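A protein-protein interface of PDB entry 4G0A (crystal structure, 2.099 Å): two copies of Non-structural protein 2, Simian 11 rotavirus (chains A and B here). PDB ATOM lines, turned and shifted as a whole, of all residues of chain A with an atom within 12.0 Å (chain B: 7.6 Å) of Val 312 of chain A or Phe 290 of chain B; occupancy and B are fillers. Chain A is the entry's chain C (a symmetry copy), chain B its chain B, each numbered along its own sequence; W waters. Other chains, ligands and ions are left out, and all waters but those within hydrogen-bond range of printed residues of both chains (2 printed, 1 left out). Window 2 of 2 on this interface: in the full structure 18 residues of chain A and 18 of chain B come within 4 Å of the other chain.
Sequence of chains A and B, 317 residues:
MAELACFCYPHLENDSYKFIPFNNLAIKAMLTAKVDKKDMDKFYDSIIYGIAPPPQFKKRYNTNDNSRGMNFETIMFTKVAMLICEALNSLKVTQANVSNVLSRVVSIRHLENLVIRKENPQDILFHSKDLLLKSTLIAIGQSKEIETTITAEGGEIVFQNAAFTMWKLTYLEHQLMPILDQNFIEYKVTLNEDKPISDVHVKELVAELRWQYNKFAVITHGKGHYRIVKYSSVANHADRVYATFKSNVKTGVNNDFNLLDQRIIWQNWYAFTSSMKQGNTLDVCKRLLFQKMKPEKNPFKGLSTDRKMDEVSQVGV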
ATOM      1  N   TRP A 211     -40.544 -11.122  35.374  1.00  0.00           N
ATOM      2  CA  TRP A 211     -39.169 -10.714  35.617  1.00  0.00           C
ATOM      3  C   TRP A 211     -38.749 -10.937  37.065  1.00  0.00           C
ATOM      4  O   TRP A 211     -37.742 -11.593  37.338  1.00  0.00           O
ATOM      5  CB  TRP A 211     -38.973  -9.244  35.246  1.00  0.00           C
ATOM      6  CG  TRP A 211     -37.624  -8.720  35.623  1.00  0.00           C
ATOM      7  CD1 TRP A 211     -37.314  -7.958  36.712  1.00  0.00           C
ATOM      8  CD2 TRP A 211     -36.394  -8.935  34.918  1.00  0.00           C
ATOM      9  NE1 TRP A 211     -35.969  -7.678  36.724  1.00  0.00           N
ATOM     10  CE2 TRP A 211     -35.382  -8.266  35.633  1.00  0.00           C
ATOM     11  CE3 TRP A 211     -36.054  -9.625  33.751  1.00  0.00           C
ATOM     12  CZ2 TRP A 211     -34.052  -8.268  35.221  1.00  0.00           C
ATOM     13  CZ3 TRP A 211     -34.732  -9.624  33.342  1.00  0.00           C
ATOM     14  CH2 TRP A 211     -33.748  -8.949  34.075  1.00  0.00           C
ATOM     15  N   LEU A 303     -41.911  -9.537  26.972  1.00  0.00           N
ATOM     16  CA  LEU A 303     -41.965  -8.631  28.115  1.00  0.00           C
ATOM     17  C   LEU A 303     -40.654  -8.618  28.893  1.00  0.00           C
ATOM     18  O   LEU A 303     -40.195  -7.564  29.338  1.00  0.00           O
ATOM     19  CB  LEU A 303     -43.124  -8.994  29.042  1.00  0.00           C
ATOM     20  CG  LEU A 303     -44.503  -8.548  28.568  1.00  0.00           C
ATOM     21  CD1 LEU A 303     -45.566  -8.925  29.580  1.00  0.00           C
ATOM     22  CD2 LEU A 303     -44.493  -7.053  28.335  1.00  0.00           C
ATOM     23  N   SER A 304     -40.054  -9.793  29.058  1.00  0.00           N
ATOM     24  CA  SER A 304     -38.794  -9.909  29.782  1.00  0.00           C
ATOM     25  C   SER A 304     -37.652  -9.271  29.000  1.00  0.00           C
ATOM     26  O   SER A 304     -36.712  -8.734  29.583  1.00  0.00           O
ATOM     27  CB  SER A 304     -38.480 -11.374  30.101  1.00  0.00           C
ATOM     28  OG  SER A 304     -38.454 -12.161  28.923  1.00  0.00           O
ATOM     29  N   THR A 305     -37.739  -9.330  27.675  1.00  0.00           N
ATOM     30  CA  THR A 305     -36.748  -8.685  26.823  1.00  0.00           C
ATOM     31  C   THR A 305     -36.718  -7.178  27.068  1.00  0.00           C
ATOM     32  O   THR A 305     -35.649  -6.580  27.170  1.00  0.00           O
ATOM     33  CB  THR A 305     -37.019  -8.955  25.335  1.00  0.00           C
ATOM     34  OG1 THR A 305     -36.893 -10.359  25.075  1.00  0.00           O
ATOM     35  CG2 THR A 305     -36.028  -8.197  24.468  1.00  0.00           C
ATOM     36  N   ASP A 306     -37.897  -6.571  27.168  1.00  0.00           N
ATOM     37  CA  ASP A 306     -37.998  -5.139  27.428  1.00  0.00           C
ATOM     38  C   ASP A 306     -37.393  -4.766  28.781  1.00  0.00           C
ATOM     39  O   ASP A 306     -36.708  -3.752  28.906  1.00  0.00           O
ATOM     40  CB  ASP A 306     -39.457  -4.681  27.362  1.00  0.00           C
ATOM     41  CG  ASP A 306     -40.051  -4.819  25.973  1.00  0.00           C
ATOM     42  OD1 ASP A 306     -39.282  -5.013  25.006  1.00  0.00           O
ATOM     43  OD2 ASP A 306     -41.290  -4.724  25.844  1.00  0.00           O
ATOM     44  N   ARG A 307     -37.654  -5.590  29.793  1.00  0.00           N
ATOM     45  CA  ARG A 307     -37.139  -5.336  31.133  1.00  0.00           C
ATOM     46  C   ARG A 307     -35.620  -5.453  31.180  1.00  0.00           C
ATOM     47  O   ARG A 307     -34.950  -4.630  31.806  1.00  0.00           O
ATOM     48  CB  ARG A 307     -37.772  -6.288  32.148  1.00  0.00           C
ATOM     49  CG  ARG A 307     -37.250  -6.108  33.562  1.00  0.00           C
ATOM     50  CD  ARG A 307     -37.467  -4.685  34.055  1.00  0.00           C
ATOM     51  NE  ARG A 307     -36.935  -4.488  35.401  1.00  0.00           N
ATOM     52  CZ  ARG A 307     -37.633  -4.680  36.515  1.00  0.00           C
ATOM     53  NH1 ARG A 307     -37.067  -4.478  37.698  1.00  0.00           N
ATOM     54  NH2 ARG A 307     -38.898  -5.076  36.447  1.00  0.00           N
ATOM     55  N   LYS A 308     -35.085  -6.482  30.524  1.00  0.00           N
ATOM     56  CA  LYS A 308     -33.640  -6.662  30.414  1.00  0.00           C
ATOM     57  C   LYS A 308     -32.995  -5.408  29.862  1.00  0.00           C
ATOM     58  O   LYS A 308     -32.021  -4.900  30.414  1.00  0.00           O
ATOM     59  CB  LYS A 308     -33.304  -7.819  29.474  1.00  0.00           C
ATOM     60  CG  LYS A 308     -33.323  -9.195  30.096  1.00  0.00           C
ATOM     61  CD  LYS A 308     -32.977 -10.240  29.044  1.00  0.00           C
ATOM     62  CE  LYS A 308     -33.261 -11.646  29.534  1.00  0.00           C
ATOM     63  NZ  LYS A 308     -33.072 -12.640  28.443  1.00  0.00           N
ATOM     64  N   MET A 309     -33.541  -4.923  28.752  1.00  0.00           N
ATOM     65  CA  MET A 309     -32.977  -3.767  28.064  1.00  0.00           C
ATOM     66  C   MET A 309     -33.055  -2.511  28.926  1.00  0.00           C
ATOM     67  O   MET A 309     -32.159  -1.671  28.887  1.00  0.00           O
ATOM     68  CB  MET A 309     -33.675  -3.550  26.719  1.00  0.00           C
ATOM     69  CG  MET A 309     -33.583  -4.753  25.790  1.00  0.00           C
ATOM     70  SD  MET A 309     -31.892  -5.357  25.584  1.00  0.00           S
ATOM     71  CE  MET A 309     -32.149  -6.722  24.453  1.00  0.00           C
ATOM     72  N   ASP A 310     -34.128  -2.391  29.703  1.00  0.00           N
ATOM     73  CA  ASP A 310     -34.255  -1.287  30.646  1.00  0.00           C
ATOM     74  C   ASP A 310     -33.181  -1.373  31.728  1.00  0.00           C
ATOM     75  O   ASP A 310     -32.598  -0.360  32.123  1.00  0.00           O
ATOM     76  CB  ASP A 310     -35.643  -1.273  31.285  1.00  0.00           C
ATOM     77  CG  ASP A 310     -36.713  -0.769  30.338  1.00  0.00           C
ATOM     78  OD1 ASP A 310     -36.381   0.014  29.423  1.00  0.00           O
ATOM     79  OD2 ASP A 310     -37.888  -1.149  30.512  1.00  0.00           O
ATOM     80  N   GLU A 311     -32.924  -2.586  32.208  1.00  0.00           N
ATOM     81  CA  GLU A 311     -31.899  -2.804  33.222  1.00  0.00           C
ATOM     82  C   GLU A 311     -30.510  -2.448  32.701  1.00  0.00           C
ATOM     83  O   GLU A 311     -29.726  -1.803  33.394  1.00  0.00           O
ATOM     84  CB  GLU A 311     -31.925  -4.256  33.709  1.00  0.00           C
ATOM     85  CG  GLU A 311     -33.172  -4.626  34.492  1.00  0.00           C
ATOM     86  CD  GLU A 311     -33.192  -4.013  35.880  1.00  0.00           C
ATOM     87  OE1 GLU A 311     -32.105  -3.752  36.436  1.00  0.00           O
ATOM     88  OE2 GLU A 311     -34.299  -3.795  36.417  1.00  0.00           O
ATOM     89  N   VAL A 312     -30.209  -2.873  31.478  1.00  0.00           N
ATOM     90  CA  VAL A 312     -28.892  -2.636  30.894  1.00  0.00           C
ATOM     91  C   VAL A 312     -28.618  -1.149  30.663  1.00  0.00           C
ATOM     92  O   VAL A 312     -27.491  -0.686  30.835  1.00  0.00           O
ATOM     93  CB  VAL A 312     -28.707  -3.402  29.570  1.00  0.00           C
ATOM     94  CG1 VAL A 312     -27.327  -3.142  29.000  1.00  0.00           C
ATOM     95  CG2 VAL A 312     -28.913  -4.888  29.792  1.00  0.00           C
ATOM     96  N   SER A 313     -29.651  -0.408  30.275  1.00  0.00           N
ATOM     97  CA  SER A 313     -29.527   1.035  30.077  1.00  0.00           C
ATOM     98  C   SER A 313     -29.131   1.747  31.369  1.00  0.00           C
ATOM     99  O   SER A 313     -29.822   1.647  32.386  1.00  0.00           O
ATOM    100  CB  SER A 313     -30.837   1.617  29.543  1.00  0.00           C
ATOM    101  OG  SER A 313     -31.215   0.990  28.331  1.00  0.00           O
ATOM    102  N   ALA B 217     -27.316 -11.573  33.510  1.00  0.00           N
ATOM    103  CA  ALA B 217     -26.737 -11.743  32.186  1.00  0.00           C
ATOM    104  C   ALA B 217     -25.585 -12.746  32.233  1.00  0.00           C
ATOM    105  O   ALA B 217     -24.755 -12.719  33.145  1.00  0.00           O
ATOM    106  CB  ALA B 217     -26.244 -10.401  31.649  1.00  0.00           C
ATOM    107  N   LYS B 230     -25.376  -9.055  37.124  1.00  0.00           N
ATOM    108  CA  LYS B 230     -26.632  -8.324  37.034  1.00  0.00           C
ATOM    109  C   LYS B 230     -26.666  -7.566  35.717  1.00  0.00           C
ATOM    110  O   LYS B 230     -25.660  -6.992  35.300  1.00  0.00           O
ATOM    111  CB  LYS B 230     -26.777  -7.347  38.201  1.00  0.00           C
ATOM    112  CG  LYS B 230     -26.991  -8.013  39.553  1.00  0.00           C
ATOM    113  CD  LYS B 230     -27.357  -6.978  40.607  1.00  0.00           C
ATOM    114  CE  LYS B 230     -27.573  -7.620  41.970  1.00  0.00           C
ATOM    115  NZ  LYS B 230     -28.042  -6.632  42.984  1.00  0.00           N
ATOM    116  N   TYR B 231     -27.815  -7.580  35.050  1.00  0.00           N
ATOM    117  CA  TYR B 231     -27.956  -6.859  33.790  1.00  0.00           C
ATOM    118  C   TYR B 231     -27.553  -5.398  33.960  1.00  0.00           C
ATOM    119  O   TYR B 231     -27.030  -4.779  33.036  1.00  0.00           O
ATOM    120  CB  TYR B 231     -29.382  -6.975  33.247  1.00  0.00           C
ATOM    121  CG  TYR B 231     -29.630  -8.264  32.497  1.00  0.00           C
ATOM    122  CD1 TYR B 231     -29.214  -8.412  31.180  1.00  0.00           C
ATOM    123  CD2 TYR B 231     -30.267  -9.335  33.108  1.00  0.00           C
ATOM    124  CE1 TYR B 231     -29.432  -9.592  30.492  1.00  0.00           C
ATOM    125  CE2 TYR B 231     -30.492 -10.517  32.426  1.00  0.00           C
ATOM    126  CZ  TYR B 231     -30.070 -10.639  31.119  1.00  0.00           C
ATOM    127  OH  TYR B 231     -30.286 -11.812  30.437  1.00  0.00           O
ATOM    128  N   SER B 232     -27.779  -4.866  35.156  1.00  0.00           N
ATOM    129  CA  SER B 232     -27.458  -3.473  35.457  1.00  0.00           C
ATOM    130  C   SER B 232     -25.956  -3.201  35.538  1.00  0.00           C
ATOM    131  O   SER B 232     -25.537  -2.050  35.663  1.00  0.00           O
ATOM    132  CB  SER B 232     -28.130  -3.046  36.764  1.00  0.00           C
ATOM    133  OG  SER B 232     -27.646  -3.808  37.855  1.00  0.00           O
ATOM    134  N   SER B 233     -25.144  -4.252  35.469  1.00  0.00           N
ATOM    135  CA  SER B 233     -23.693  -4.088  35.555  1.00  0.00           C
ATOM    136  C   SER B 233     -23.004  -4.353  34.217  1.00  0.00           C
ATOM    137  O   SER B 233     -21.794  -4.166  34.082  1.00  0.00           O
ATOM    138  CB  SER B 233     -23.113  -5.010  36.633  1.00  0.00           C
ATOM    139  OG  SER B 233     -22.994  -6.341  36.150  1.00  0.00           O
ATOM    140  N   VAL B 234     -23.783  -4.780  33.228  1.00  0.00           N
ATOM    141  CA  VAL B 234     -23.231  -5.211  31.945  1.00  0.00           C
ATOM    142  C   VAL B 234     -22.419  -4.134  31.215  1.00  0.00           C
ATOM    143  O   VAL B 234     -21.329  -4.410  30.710  1.00  0.00           O
ATOM    144  CB  VAL B 234     -24.333  -5.760  31.013  1.00  0.00           C
ATOM    145  CG1 VAL B 234     -23.772  -6.034  29.631  1.00  0.00           C
ATOM    146  CG2 VAL B 234     -24.938  -7.025  31.602  1.00  0.00           C
ATOM    147  N   ALA B 235     -22.949  -2.914  31.156  1.00  0.00           N
ATOM    148  CA  ALA B 235     -22.267  -1.823  30.459  1.00  0.00           C
ATOM    149  C   ALA B 235     -20.879  -1.577  31.042  1.00  0.00           C
ATOM    150  O   ALA B 235     -19.926  -1.300  30.311  1.00  0.00           O
ATOM    151  CB  ALA B 235     -23.103  -0.547  30.500  1.00  0.00           C
ATOM    152  N   ASN B 236     -20.770  -1.685  32.362  1.00  0.00           N
ATOM    153  CA  ASN B 236     -19.485  -1.530  33.034  1.00  0.00           C
ATOM    154  C   ASN B 236     -18.519  -2.657  32.679  1.00  0.00           C
ATOM    155  O   ASN B 236     -17.334  -2.416  32.445  1.00  0.00           O
ATOM    156  CB  ASN B 236     -19.674  -1.446  34.551  1.00  0.00           C
ATOM    157  CG  ASN B 236     -18.356  -1.398  35.300  1.00  0.00           C
ATOM    158  OD1 ASN B 236     -17.875  -2.415  35.801  1.00  0.00           O
ATOM    159  ND2 ASN B 236     -17.762  -0.212  35.375  1.00  0.00           N
ATOM    160  N   ALA B 238     -18.596  -4.286  29.937  1.00  0.00           N
ATOM    161  CA  ALA B 238     -18.247  -4.021  28.548  1.00  0.00           C
ATOM    162  C   ALA B 238     -17.061  -3.069  28.454  1.00  0.00           C
ATOM    163  O   ALA B 238     -16.140  -3.292  27.668  1.00  0.00           O
ATOM    164  CB  ALA B 238     -19.441  -3.458  27.801  1.00  0.00           C
ATOM    165  N   ASP B 239     -17.089  -2.011  29.262  1.00  0.00           N
ATOM    166  CA  ASP B 239     -16.014  -1.022  29.273  1.00  0.00           C
ATOM    167  C   ASP B 239     -14.690  -1.636  29.706  1.00  0.00           C
ATOM    168  O   ASP B 239     -13.657  -1.409  29.075  1.00  0.00           O
ATOM    169  CB  ASP B 239     -16.363   0.160  30.186  1.00  0.00           C
ATOM    170  CG  ASP B 239     -17.452   1.040  29.610  1.00  0.00           C
ATOM    171  OD1 ASP B 239     -17.682   0.965  28.387  1.00  0.00           O
ATOM    172  OD2 ASP B 239     -18.073   1.809  30.375  1.00  0.00           O
ATOM    173  N   TRP B 266     -25.401 -14.396  26.775  1.00  0.00           N
ATOM    174  CA  TRP B 266     -26.455 -13.449  26.414  1.00  0.00           C
ATOM    175  C   TRP B 266     -26.237 -12.929  24.993  1.00  0.00           C
ATOM    176  O   TRP B 266     -25.135 -12.512  24.638  1.00  0.00           O
ATOM    177  CB  TRP B 266     -26.476 -12.272  27.393  1.00  0.00           C
ATOM    178  CG  TRP B 266     -27.576 -11.285  27.131  1.00  0.00           C
ATOM    179  CD1 TRP B 266     -28.857 -11.565  26.748  1.00  0.00           C
ATOM    180  CD2 TRP B 266     -27.490  -9.856  27.229  1.00  0.00           C
ATOM    181  NE1 TRP B 266     -29.575 -10.400  26.604  1.00  0.00           N
ATOM    182  CE2 TRP B 266     -28.758  -9.338  26.893  1.00  0.00           C
ATOM    183  CE3 TRP B 266     -26.464  -8.966  27.564  1.00  0.00           C
ATOM    184  CZ2 TRP B 266     -29.028  -7.970  26.884  1.00  0.00           C
ATOM    185  CZ3 TRP B 266     -26.735  -7.607  27.557  1.00  0.00           C
ATOM    186  CH2 TRP B 266     -28.006  -7.123  27.218  1.00  0.00           C
ATOM    187  N   ASN B 268     -26.870 -10.216  23.308  1.00  0.00           N
ATOM    188  CA  ASN B 268     -26.265  -8.898  23.142  1.00  0.00           C
ATOM    189  C   ASN B 268     -24.780  -8.872  23.488  1.00  0.00           C
ATOM    190  O   ASN B 268     -24.001  -8.178  22.836  1.00  0.00           O
ATOM    191  CB  ASN B 268     -27.020  -7.850  23.953  1.00  0.00           C
ATOM    192  CG  ASN B 268     -28.437  -7.642  23.453  1.00  0.00           C
ATOM    193  OD1 ASN B 268     -29.271  -8.547  23.519  1.00  0.00           O
ATOM    194  ND2 ASN B 268     -28.718  -6.446  22.955  1.00  0.00           N
ATOM    195  N   PHE B 272     -21.735  -7.961  20.960  1.00  0.00           N
ATOM    196  CA  PHE B 272     -20.776  -6.937  21.360  1.00  0.00           C
ATOM    197  C   PHE B 272     -19.332  -7.423  21.292  1.00  0.00           C
ATOM    198  O   PHE B 272     -18.478  -6.765  20.698  1.00  0.00           O
ATOM    199  CB  PHE B 272     -21.109  -6.419  22.761  1.00  0.00           C
ATOM    200  CG  PHE B 272     -19.931  -5.854  23.502  1.00  0.00           C
ATOM    201  CD1 PHE B 272     -19.372  -4.641  23.131  1.00  0.00           C
ATOM    202  CD2 PHE B 272     -19.394  -6.527  24.588  1.00  0.00           C
ATOM    203  CE1 PHE B 272     -18.292  -4.119  23.819  1.00  0.00           C
ATOM    204  CE2 PHE B 272     -18.318  -6.010  25.281  1.00  0.00           C
ATOM    205  CZ  PHE B 272     -17.763  -4.805  24.896  1.00  0.00           C
ATOM    206  N   ASP B 283     -17.696   2.553  20.396  1.00  0.00           N
ATOM    207  CA  ASP B 283     -19.014   3.090  20.072  1.00  0.00           C
ATOM    208  C   ASP B 283     -19.842   2.097  19.266  1.00  0.00           C
ATOM    209  O   ASP B 283     -21.026   1.900  19.539  1.00  0.00           O
ATOM    210  CB  ASP B 283     -18.892   4.410  19.305  1.00  0.00           C
ATOM    211  CG  ASP B 283     -18.434   5.555  20.185  1.00  0.00           C
ATOM    212  OD1 ASP B 283     -18.731   5.529  21.397  1.00  0.00           O
ATOM    213  OD2 ASP B 283     -17.781   6.483  19.662  1.00  0.00           O
ATOM    214  N   CYS B 285     -19.201  -1.313  18.909  1.00  0.00           N
ATOM    215  CA  CYS B 285     -19.356  -2.528  19.707  1.00  0.00           C
ATOM    216  C   CYS B 285     -20.424  -2.352  20.779  1.00  0.00           C
ATOM    217  O   CYS B 285     -21.390  -3.114  20.855  1.00  0.00           O
ATOM    218  CB  CYS B 285     -18.026  -2.892  20.386  1.00  0.00           C
ATOM    219  SG  CYS B 285     -16.683  -3.293  19.264  1.00  0.00           S
ATOM    220  N   LYS B 286     -20.239  -1.326  21.601  1.00  0.00           N
ATOM    221  CA  LYS B 286     -21.032  -1.138  22.808  1.00  0.00           C
ATOM    222  C   LYS B 286     -22.512  -0.866  22.544  1.00  0.00           C
ATOM    223  O   LYS B 286     -23.362  -1.233  23.354  1.00  0.00           O
ATOM    224  CB  LYS B 286     -20.428  -0.021  23.660  1.00  0.00           C
ATOM    225  CG  LYS B 286     -20.911   0.007  25.098  1.00  0.00           C
ATOM    226  CD  LYS B 286     -20.173   1.069  25.890  1.00  0.00           C
ATOM    227  CE  LYS B 286     -20.712   1.186  27.305  1.00  0.00           C
ATOM    228  NZ  LYS B 286     -20.079   2.322  28.030  1.00  0.00           N
ATOM    229  N   ARG B 287     -22.827  -0.226  21.422  1.00  0.00           N
ATOM    230  CA  ARG B 287     -24.225   0.091  21.137  1.00  0.00           C
ATOM    231  C   ARG B 287     -25.055  -1.169  20.891  1.00  0.00           C
ATOM    232  O   ARG B 287     -26.274  -1.159  21.051  1.00  0.00           O
ATOM    233  CB  ARG B 287     -24.365   1.089  19.979  1.00  0.00           C
ATOM    234  CG  ARG B 287     -23.789   0.640  18.649  1.00  0.00           C
ATOM    235  CD  ARG B 287     -24.185   1.617  17.546  1.00  0.00           C
ATOM    236  NE  ARG B 287     -24.052   3.005  17.982  1.00  0.00           N
ATOM    237  CZ  ARG B 287     -23.181   3.875  17.476  1.00  0.00           C
ATOM    238  NH1 ARG B 287     -22.362   3.514  16.496  1.00  0.00           N
ATOM    239  NH2 ARG B 287     -23.138   5.115  17.946  1.00  0.00           N
ATOM    240  N   LEU B 288     -24.387  -2.256  20.520  1.00  0.00           N
ATOM    241  CA  LEU B 288     -25.065  -3.534  20.329  1.00  0.00           C
ATOM    242  C   LEU B 288     -25.623  -4.070  21.652  1.00  0.00           C
ATOM    243  O   LEU B 288     -26.542  -4.891  21.664  1.00  0.00           O
ATOM    244  CB  LEU B 288     -24.125  -4.554  19.681  1.00  0.00           C
ATOM    245  CG  LEU B 288     -23.616  -4.201  18.280  1.00  0.00           C
ATOM    246  CD1 LEU B 288     -22.560  -5.198  17.815  1.00  0.00           C
ATOM    247  CD2 LEU B 288     -24.766  -4.122  17.280  1.00  0.00           C
ATOM    248  N   LEU B 289     -25.069  -3.594  22.764  1.00  0.00           N
ATOM    249  CA  LEU B 289     -25.560  -3.973  24.087  1.00  0.00           C
ATOM    250  C   LEU B 289     -26.952  -3.415  24.359  1.00  0.00           C
ATOM    251  O   LEU B 289     -27.730  -4.009  25.105  1.00  0.00           O
ATOM    252  CB  LEU B 289     -24.611  -3.480  25.182  1.00  0.00           C
ATOM    253  CG  LEU B 289     -23.258  -4.153  25.398  1.00  0.00           C
ATOM    254  CD1 LEU B 289     -22.571  -3.510  26.588  1.00  0.00           C
ATOM    255  CD2 LEU B 289     -23.416  -5.648  25.622  1.00  0.00           C
ATOM    256  N   PHE B 290     -27.259  -2.267  23.762  1.00  0.00           N
ATOM    257  CA  PHE B 290     -28.492  -1.551  24.079  1.00  0.00           C
ATOM    258  C   PHE B 290     -29.578  -1.723  23.020  1.00  0.00           C
ATOM    259  O   PHE B 290     -30.646  -1.120  23.117  1.00  0.00           O
ATOM    260  CB  PHE B 290     -28.202  -0.062  24.283  1.00  0.00           C
ATOM    261  CG  PHE B 290     -27.116   0.214  25.280  1.00  0.00           C
ATOM    262  CD1 PHE B 290     -27.378   0.175  26.639  1.00  0.00           C
ATOM    263  CD2 PHE B 290     -25.832   0.519  24.859  1.00  0.00           C
ATOM    264  CE1 PHE B 290     -26.380   0.430  27.560  1.00  0.00           C
ATOM    265  CE2 PHE B 290     -24.829   0.776  25.776  1.00  0.00           C
ATOM    266  CZ  PHE B 290     -25.103   0.731  27.127  1.00  0.00           C
ATOM    267  N   GLN B 291     -29.302  -2.540  22.010  1.00  0.00           N
ATOM    268  CA  GLN B 291     -30.263  -2.764  20.938  1.00  0.00           C
ATOM    269  C   GLN B 291     -31.153  -3.968  21.221  1.00  0.00           C
ATOM    270  O   GLN B 291     -30.664  -5.049  21.550  1.00  0.00           O
ATOM    271  CB  GLN B 291     -29.548  -2.963  19.602  1.00  0.00           C
ATOM    272  CG  GLN B 291     -28.716  -1.776  19.147  1.00  0.00           C
ATOM    273  CD  GLN B 291     -28.162  -1.961  17.746  1.00  0.00           C
ATOM    274  OE1 GLN B 291     -28.629  -2.817  16.990  1.00  0.00           O
ATOM    275  NE2 GLN B 291     -27.160  -1.163  17.394  1.00  0.00           N
ATOM    276  N   LYS B 292     -32.460  -3.774  21.093  1.00  0.00           N
ATOM    277  CA  LYS B 292     -33.403  -4.879  21.188  1.00  0.00           C
ATOM    278  C   LYS B 292     -33.253  -5.726  19.934  1.00  0.00           C
ATOM    279  O   LYS B 292     -33.621  -5.297  18.841  1.00  0.00           O
ATOM    280  CB  LYS B 292     -34.832  -4.351  21.301  1.00  0.00           C
ATOM    281  CG  LYS B 292     -35.830  -5.367  21.822  1.00  0.00           C
ATOM    282  CD  LYS B 292     -36.399  -4.922  23.158  1.00  0.00           C
ATOM    283  CE  LYS B 292     -37.014  -3.534  23.052  1.00  0.00           C
ATOM    284  NZ  LYS B 292     -37.532  -3.048  24.358  1.00  0.00           N
ATOM    285  N   MET B 293     -32.707  -6.926  20.090  1.00  0.00           N
ATOM    286  CA  MET B 293     -32.353  -7.751  18.939  1.00  0.00           C
ATOM    287  C   MET B 293     -33.454  -8.715  18.518  1.00  0.00           C
ATOM    288  O   MET B 293     -34.287  -9.124  19.328  1.00  0.00           O
ATOM    289  CB  MET B 293     -31.067  -8.533  19.217  1.00  0.00           C
ATOM    290  CG  MET B 293     -29.827  -7.668  19.324  1.00  0.00           C
ATOM    291  SD  MET B 293     -28.334  -8.633  19.621  1.00  0.00           S
ATOM    292  CE  MET B 293     -27.102  -7.336  19.566  1.00  0.00           C
HETATM  293  O   HOH W   1     -37.362  -1.475  26.500  1.00  0.00           O
HETATM  294  O   HOH W   2     -30.043  -5.846  36.989  1.00  0.00           O
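Of the printed residues of chain B, Asp 306 of chain A touches Lys 292 (2.7 Å).
Of the printed residues of chain B, Lys 308 of chain A touches Tyr 231.
Printed residues of chain B within 4 Å of Glu 311 of chain A: Tyr 231 (3.8 Å) and Ser 232 (3.5 Å).
Of the printed residues of chain B, Val 312 of chain A touches Tyr 231, Trp 266 and Phe 290.
Of chain A, only Glu 311 (3.5 Å) comes within 4 Å of Ser 232 of chain B.
No residue of chain A comes within 4 Å of Val 234 of chain B.
No residue of chain A comes within 4 Å of Ala 235 of chain B.
Of the printed residues of chain A, Asn 268 of chain B touches Met 309 (3.5 Å).
No residue of chain A comes within 4 Å of Lys 286 of chain B.
Leu 288 of chain B touches none of the printed residues of chain A.
Phe 290 of chain B touches just one residue of chain A: Val 312 (3.6 Å).
Of chain A, only Met 309 (3.7 Å) comes within 4 Å of Gln 291 of chain B.
Of chain A, only Thr 305 (3.5 Å), Asp 306 (2.7 Å) and Met 309 (3.9 Å) come within 4 Å of Lys 292 of chain B.
The nearest residue of chain A that does not touch Phe 290 of chain B is Ser 313 of chain A (4.1 Å).
Of the 23 printed residues of chain B, 7 touch a printed residue of chain A.
Hydrophobic or aromatic side chains of chain B within 4 Å of the printed part of chain A: Tyr 231, Trp 266 and Phe 290.
Along chain B the printed residues that touch a printed residue of chain A span positions 231 to 292.
Of the 12 printed residues of chain A, 7 touch a printed residue of chain B.
Printed residues of chain A that touch a printed residue of chain B: Trp 211, Thr 305, Asp 306, Lys 308, Met 309, Glu 311 and Val 312.
Hydrophobic or aromatic side chains of chain A within 4 Å of the printed part of chain B: Trp 211, Met 309 and Val 312.
The guanidinium group (NE) of Arg 307 of chain A is in salt-bridge range of the side-chain carboxylate (OE2) of Glu 311 of chain A.
O of Met 309 of chain A lies within hydrogen-bond range of OG of Ser 313 of chain A (2.9 Å).
ND2 of Asn 268 of chain B sits at hydrogen-bond distance from O of Gln 291 of chain B (2.8 Å).
ND2 of Asn 268 of chain B is in hydrogen-bond range of O of Leu 288 of chain B.
ND2 of Asn 268 of chain B lies within hydrogen-bond range of O of Leu 289 of chain B (3.4 Å).
Water W1 lies within hydrogen-bond range of NZ of Lys 292 of chain B, O of Asp 306 of chain A and OD1 of Asp 310 of chain A.
Water W2 lies within hydrogen-bond range of OE1 of Glu 311 of chain A (3.0 Å), N of Ser 232 of chain B (3.1 Å) and N of Tyr 231 of chain B (3.4 Å).
No position is printed for both chains.
Of the 12 pairs that touch across the chains among the printed residues, none has its exchanged pair printed and touching as well.
The side-chain amino group of Lys 292 of chain B lies within salt-bridge range of the side-chain carboxylate of Asp 306 of chain A (2.7 Å).
Among the printed residues, pairs that only touch across the chains: Trp 211 of chain A with Tyr 231 of chain B (3.6 Å), Thr 305 of chain A with Lys 292 of chain B (3.5 Å), Lys 308 of chain A with Tyr 231 of chain B (3.1 Å), Met 309 of chain A with Asn 268 of chain B (3.5 Å), Met 309 of chain A with Gln 291 of chain B (3.7 Å), Met 309 of chain A with Lys 292 of chain B (3.9 Å), Glu 311 of chain A with Tyr 231 of chain B (3.8 Å), Glu 311 of chain A with Ser 232 of chain B (3.5 Å), Val 312 of chain A with Tyr 231 of chain B (3.6 Å), Val 312 of chain A with Trp 266 of chain B (3.5 Å) and Val 312 of chain A with Phe 290 of chain B (3.6 Å).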
